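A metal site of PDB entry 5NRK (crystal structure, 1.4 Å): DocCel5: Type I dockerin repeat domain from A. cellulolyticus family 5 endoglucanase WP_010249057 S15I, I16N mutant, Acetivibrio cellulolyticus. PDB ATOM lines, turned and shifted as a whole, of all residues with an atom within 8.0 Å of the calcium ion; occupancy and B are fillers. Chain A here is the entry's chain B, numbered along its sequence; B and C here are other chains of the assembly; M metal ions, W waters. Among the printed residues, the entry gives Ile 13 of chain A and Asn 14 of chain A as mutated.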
ATOM      1  N   LYS A   1     -14.697  19.068  17.079  1.00  0.00           N
ATOM      2  CA  LYS A   1     -14.822  18.975  18.573  1.00  0.00           C
ATOM      3  C   LYS A   1     -15.879  20.017  18.989  1.00  0.00           C
ATOM      4  O   LYS A   1     -16.992  19.639  19.258  1.00  0.00           O
ATOM      5  CB  LYS A   1     -13.467  19.089  19.299  1.00  0.00           C
ATOM      6  CG  LYS A   1     -13.478  18.836  20.812  1.00  0.00           C
ATOM      7  CD  LYS A   1     -13.947  17.451  21.176  1.00  0.00           C
ATOM      8  CE  LYS A   1     -12.818  16.568  21.678  1.00  0.00           C
ATOM      9  NZ  LYS A   1     -11.751  16.315  20.668  1.00  0.00           N
ATOM     10  N   GLY A   3     -19.030  22.106  18.920  1.00  0.00           N
ATOM     11  CA  GLY A   3     -20.240  21.873  18.152  1.00  0.00           C
ATOM     12  C   GLY A   3     -20.736  20.431  18.222  1.00  0.00           C
ATOM     13  O   GLY A   3     -21.917  20.196  17.986  1.00  0.00           O
ATOM     14  N   ASP A   4     -19.851  19.503  18.560  1.00  0.00           N
ATOM     15  CA  ASP A   4     -20.217  18.089  18.555  1.00  0.00           C
ATOM     16  C   ASP A   4     -20.633  17.737  19.977  1.00  0.00           C
ATOM     17  O   ASP A   4     -19.893  17.099  20.726  1.00  0.00           O
ATOM     18  CB  ASP A   4     -19.036  17.264  18.075  1.00  0.00           C
ATOM     19  CG  ASP A   4     -19.313  15.777  18.063  1.00  0.00           C
ATOM     20  OD1 ASP A   4     -20.506  15.384  18.061  1.00  0.00           O
ATOM     21  OD2 ASP A   4     -18.346  15.006  18.090  1.00  0.00           O
ATOM     22  N   VAL A   5     -21.833  18.176  20.339  1.00  0.00           N
ATOM     23  CA  VAL A   5     -22.266  18.027  21.723  1.00  0.00           C
ATOM     24  C   VAL A   5     -22.615  16.608  22.127  1.00  0.00           C
ATOM     25  O   VAL A   5     -22.647  16.329  23.325  1.00  0.00           O
ATOM     26  CB  VAL A   5     -23.374  19.024  22.100  1.00  0.00           C
ATOM     27  CG1 VAL A   5     -22.851  20.452  22.019  1.00  0.00           C
ATOM     28  CG2 VAL A   5     -24.613  18.842  21.251  1.00  0.00           C
ATOM     29  N   ASP A   6     -22.849  15.702  21.180  1.00  0.00           N
ATOM     30  CA  ASP A   6     -22.949  14.289  21.549  1.00  0.00           C
ATOM     31  C   ASP A   6     -21.631  13.523  21.399  1.00  0.00           C
ATOM     32  O   ASP A   6     -21.586  12.330  21.677  1.00  0.00           O
ATOM     33  CB  ASP A   6     -24.136  13.584  20.884  1.00  0.00           C
ATOM     34  CG  ASP A   6     -24.070  13.541  19.407  1.00  0.00           C
ATOM     35  OD1 ASP A   6     -23.096  13.975  18.809  1.00  0.00           O
ATOM     36  OD2 ASP A   6     -25.035  13.008  18.831  1.00  0.00           O
ATOM     37  N   GLY A   7     -20.573  14.214  20.990  1.00  0.00           N
ATOM     38  CA  GLY A   7     -19.252  13.594  20.939  1.00  0.00           C
ATOM     39  C   GLY A   7     -19.157  12.428  19.977  1.00  0.00           C
ATOM     40  O   GLY A   7     -18.345  11.522  20.172  1.00  0.00           O
ATOM     41  N   ASN A   8     -19.983  12.436  18.927  1.00  0.00           N
ATOM     42  CA  ASN A   8     -19.968  11.320  17.976  1.00  0.00           C
ATOM     43  C   ASN A   8     -19.127  11.548  16.732  1.00  0.00           C
ATOM     44  O   ASN A   8     -19.140  10.697  15.840  1.00  0.00           O
ATOM     45  CB  ASN A   8     -21.391  10.913  17.574  1.00  0.00           C
ATOM     46  CG  ASN A   8     -22.039  11.871  16.590  1.00  0.00           C
ATOM     47  OD1 ASN A   8     -21.633  13.039  16.417  1.00  0.00           O
ATOM     48  ND2 ASN A   8     -23.109  11.406  15.994  1.00  0.00           N
ATOM     49  N   GLY A   9     -18.396  12.658  16.673  1.00  0.00           N
ATOM     50  CA  GLY A   9     -17.514  12.958  15.551  1.00  0.00           C
ATOM     51  C   GLY A   9     -18.098  13.747  14.399  1.00  0.00           C
ATOM     52  O   GLY A   9     -17.368  14.124  13.466  1.00  0.00           O
ATOM     53  N   SER A  10     -19.404  14.000  14.428  1.00  0.00           N
ATOM     54  CA  SER A  10     -20.068  14.764  13.388  1.00  0.00           C
ATOM     55  C   SER A  10     -20.763  15.949  14.032  1.00  0.00           C
ATOM     56  O   SER A  10     -21.171  15.860  15.169  1.00  0.00           O
ATOM     57  CB  SER A  10     -21.131  13.919  12.686  1.00  0.00           C
ATOM     58  OG  SER A  10     -20.603  12.729  12.122  1.00  0.00           O
ATOM     59  N   ILE A  11     -20.898  17.053  13.298  1.00  0.00           N
ATOM     60  CA  ILE A  11     -21.704  18.196  13.732  1.00  0.00           C
ATOM     61  C   ILE A  11     -22.892  18.306  12.788  1.00  0.00           C
ATOM     62  O   ILE A  11     -22.717  18.590  11.594  1.00  0.00           O
ATOM     63  CB  ILE A  11     -20.903  19.519  13.734  1.00  0.00           C
ATOM     64  CG1 ILE A  11     -19.675  19.376  14.639  1.00  0.00           C
ATOM     65  CG2 ILE A  11     -21.788  20.660  14.195  1.00  0.00           C
ATOM     66  CD1 ILE A  11     -18.618  20.442  14.396  1.00  0.00           C
ATOM     67  N   ASN A  12     -24.089  18.091  13.296  1.00  0.00           N
ATOM     68  CA  ASN A  12     -25.260  17.986  12.452  1.00  0.00           C
ATOM     69  C   ASN A  12     -26.555  18.329  13.222  1.00  0.00           C
ATOM     70  O   ASN A  12     -26.518  18.832  14.336  1.00  0.00           O
ATOM     71  CB  ASN A  12     -25.312  16.590  11.827  1.00  0.00           C
ATOM     72  CG  ASN A  12     -25.364  15.468  12.859  1.00  0.00           C
ATOM     73  OD1 ASN A  12     -25.995  15.616  13.928  1.00  0.00           O
ATOM     74  ND2 ASN A  12     -24.748  14.352  12.549  1.00  0.00           N
ATOM     75  N   ILE A  13     -27.693  18.069  12.574  1.00  0.00           N
ATOM     76  CA  ILE A  13     -29.002  18.344  13.107  1.00  0.00           C
ATOM     77  C   ILE A  13     -29.184  17.825  14.525  1.00  0.00           C
ATOM     78  O   ILE A  13     -29.885  18.435  15.314  1.00  0.00           O
ATOM     79  CB  ILE A  13     -30.134  17.776  12.181  1.00  0.00           C
ATOM     80  CG1 ILE A  13     -31.528  18.168  12.692  1.00  0.00           C
ATOM     81  CG2 ILE A  13     -30.018  16.271  12.007  1.00  0.00           C
ATOM     82  CD1 ILE A  13     -32.640  17.847  11.710  1.00  0.00           C
ATOM     83  N   ASN A  14     -28.592  16.683  14.849  1.00  0.00           N
ATOM     84  CA  ASN A  14     -28.798  16.125  16.175  1.00  0.00           C
ATOM     85  C   ASN A  14     -28.086  16.904  17.260  1.00  0.00           C
ATOM     86  O   ASN A  14     -28.562  16.973  18.384  1.00  0.00           O
ATOM     87  CB  ASN A  14     -28.415  14.647  16.186  1.00  0.00           C
ATOM     88  CG  ASN A  14     -29.325  13.823  15.304  1.00  0.00           C
ATOM     89  OD1 ASN A  14     -30.452  14.233  14.999  1.00  0.00           O
ATOM     90  ND2 ASN A  14     -28.846  12.670  14.879  1.00  0.00           N
ATOM     91  N   ASP A  15     -26.930  17.492  16.934  1.00  0.00           N
ATOM     92  CA  ASP A  15     -26.283  18.385  17.883  1.00  0.00           C
ATOM     93  C   ASP A  15     -27.157  19.619  18.127  1.00  0.00           C
ATOM     94  O   ASP A  15     -27.243  20.115  19.252  1.00  0.00           O
ATOM     95  CB  ASP A  15     -24.913  18.783  17.366  1.00  0.00           C
ATOM     96  CG  ASP A  15     -23.995  17.583  17.206  1.00  0.00           C
ATOM     97  OD1 ASP A  15     -23.555  16.962  18.191  1.00  0.00           O
ATOM     98  OD2 ASP A  15     -23.734  17.193  16.051  1.00  0.00           O
ATOM     99  N   PHE A  16     -27.822  20.115  17.070  1.00  0.00           N
ATOM    100  CA  PHE A  16     -28.744  21.246  17.213  1.00  0.00           C
ATOM    101  C   PHE A  16     -29.940  20.880  18.099  1.00  0.00           C
ATOM    102  O   PHE A  16     -30.325  21.646  18.985  1.00  0.00           O
ATOM    103  CB  PHE A  16     -29.176  21.708  15.815  1.00  0.00           C
ATOM    104  CG  PHE A  16     -30.033  22.951  15.808  1.00  0.00           C
ATOM    105  CD1 PHE A  16     -29.500  24.215  16.026  1.00  0.00           C
ATOM    106  CD2 PHE A  16     -31.382  22.850  15.528  1.00  0.00           C
ATOM    107  CE1 PHE A  16     -30.325  25.353  15.998  1.00  0.00           C
ATOM    108  CE2 PHE A  16     -32.191  23.978  15.461  1.00  0.00           C
ATOM    109  CZ  PHE A  16     -31.658  25.223  15.720  1.00  0.00           C
ATOM    110  N   LEU A  18     -30.012  18.529  20.377  1.00  0.00           N
ATOM    111  CA  LEU A  18     -29.525  18.383  21.734  1.00  0.00           C
ATOM    112  C   LEU A  18     -29.373  19.736  22.406  1.00  0.00           C
ATOM    113  O   LEU A  18     -29.738  19.906  23.575  1.00  0.00           O
ATOM    114  CB  LEU A  18     -28.180  17.628  21.747  1.00  0.00           C
ATOM    115  CG  LEU A  18     -28.273  16.144  21.468  1.00  0.00           C
ATOM    116  CD1 LEU A  18     -26.905  15.597  21.088  1.00  0.00           C
ATOM    117  CD2 LEU A  18     -28.832  15.389  22.675  1.00  0.00           C
ATOM    118  N   MET A  55     -24.461  27.698  16.212  1.00  0.00           N
ATOM    119  CA  MET A  55     -24.658  26.379  15.625  1.00  0.00           C
ATOM    120  C   MET A  55     -25.624  26.432  14.437  1.00  0.00           C
ATOM    121  O   MET A  55     -25.394  25.781  13.415  1.00  0.00           O
ATOM    122  CB  MET A  55     -25.174  25.425  16.689  1.00  0.00           C
ATOM    123  CG  MET A  55     -25.329  24.032  16.133  1.00  0.00           C
ATOM    124  SD  MET A  55     -25.760  22.759  17.316  1.00  0.00           S
ATOM    125  CE  MET A  55     -24.451  22.678  18.518  1.00  0.00           C
ATOM    126  N   GLY B  63     -23.632   8.632  12.143  1.00  0.00           N
ATOM    127  CA  GLY B  63     -23.461   9.968  12.699  1.00  0.00           C
ATOM    128  C   GLY B  63     -24.735  10.776  12.785  1.00  0.00           C
ATOM    129  O   GLY B  63     -24.842  11.638  13.657  1.00  0.00           O
ATOM    130  N   VAL B  64     -25.683  10.492  11.908  1.00  0.00           N
ATOM    131  CA  VAL B  64     -27.013  11.087  11.927  1.00  0.00           C
ATOM    132  C   VAL B  64     -28.073  10.082  12.422  1.00  0.00           C
ATOM    133  O   VAL B  64     -28.951  10.416  13.225  1.00  0.00           O
ATOM    134  CB  VAL B  64     -27.359  11.524  10.475  1.00  0.00           C
ATOM    135  CG1 VAL B  64     -28.792  12.009  10.327  1.00  0.00           C
ATOM    136  CG2 VAL B  64     -26.382  12.608   9.985  1.00  0.00           C
ATOM    137  N   ARG C  20     -37.245  13.108  19.435  1.00  0.00           N
ATOM    138  CA  ARG C  20     -35.966  12.433  19.585  1.00  0.00           C
ATOM    139  C   ARG C  20     -35.551  12.327  21.058  1.00  0.00           C
ATOM    140  O   ARG C  20     -35.141  11.271  21.551  1.00  0.00           O
ATOM    141  CB  ARG C  20     -34.877  13.156  18.774  1.00  0.00           C
ATOM    142  CG  ARG C  20     -33.590  12.353  18.706  1.00  0.00           C
ATOM    143  CD  ARG C  20     -32.553  12.987  17.787  1.00  0.00           C
ATOM    144  NE  ARG C  20     -31.383  12.128  17.594  1.00  0.00           N
ATOM    145  CZ  ARG C  20     -30.293  12.099  18.368  1.00  0.00           C
ATOM    146  NH1 ARG C  20     -30.131  12.922  19.386  1.00  0.00           N
ATOM    147  NH2 ARG C  20     -29.334  11.209  18.087  1.00  0.00           N
HETATM  148 CA    CA M   1     -22.540  15.163  16.934  1.00  0.00          CA
HETATM  149  O   HOH W   1     -24.501  14.247  15.935  1.00  0.00           O
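The calcium ion is bound by OD1 of Asp 6 (2.3 Å).
OD1 of Asp 4 is bound to the calcium ion (2.3 Å).
The calcium ion is bound by O of Ser 10, at 2.3 Å.
OD1 of Asn 8 binds the calcium ion (2.4 Å).
Water W1 binds the calcium ion.
The calcium ion is bound by OD1 of Asp 15 (2.4 Å).
The calcium ion is bound by OD2 of Asp 15, at 2.5 Å.
The backbone NH (N) of Gly 7 sits close to the side-chain carboxylate (OD1) of Asp 4 (3.2 Å).
OD2 of Asp 4 is in hydrogen-bond range of N of Gly 9, at 2.7 Å.
ND2 of Asn 8 lies within hydrogen-bond range of O of Gly 63 of chain B, 2.9 Å away.
N of Val 5 sits close to OD1 of Asp 15 (3.0 Å).
The backbone NH (N) of Asn 12 lies close to the side-chain carboxylate (OD2) of Asp 15.
Five residues have an atom within 4 Å of the calcium ion: Asp 4, Asp 6, Asn 8, Ser 10 and Asp 15.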
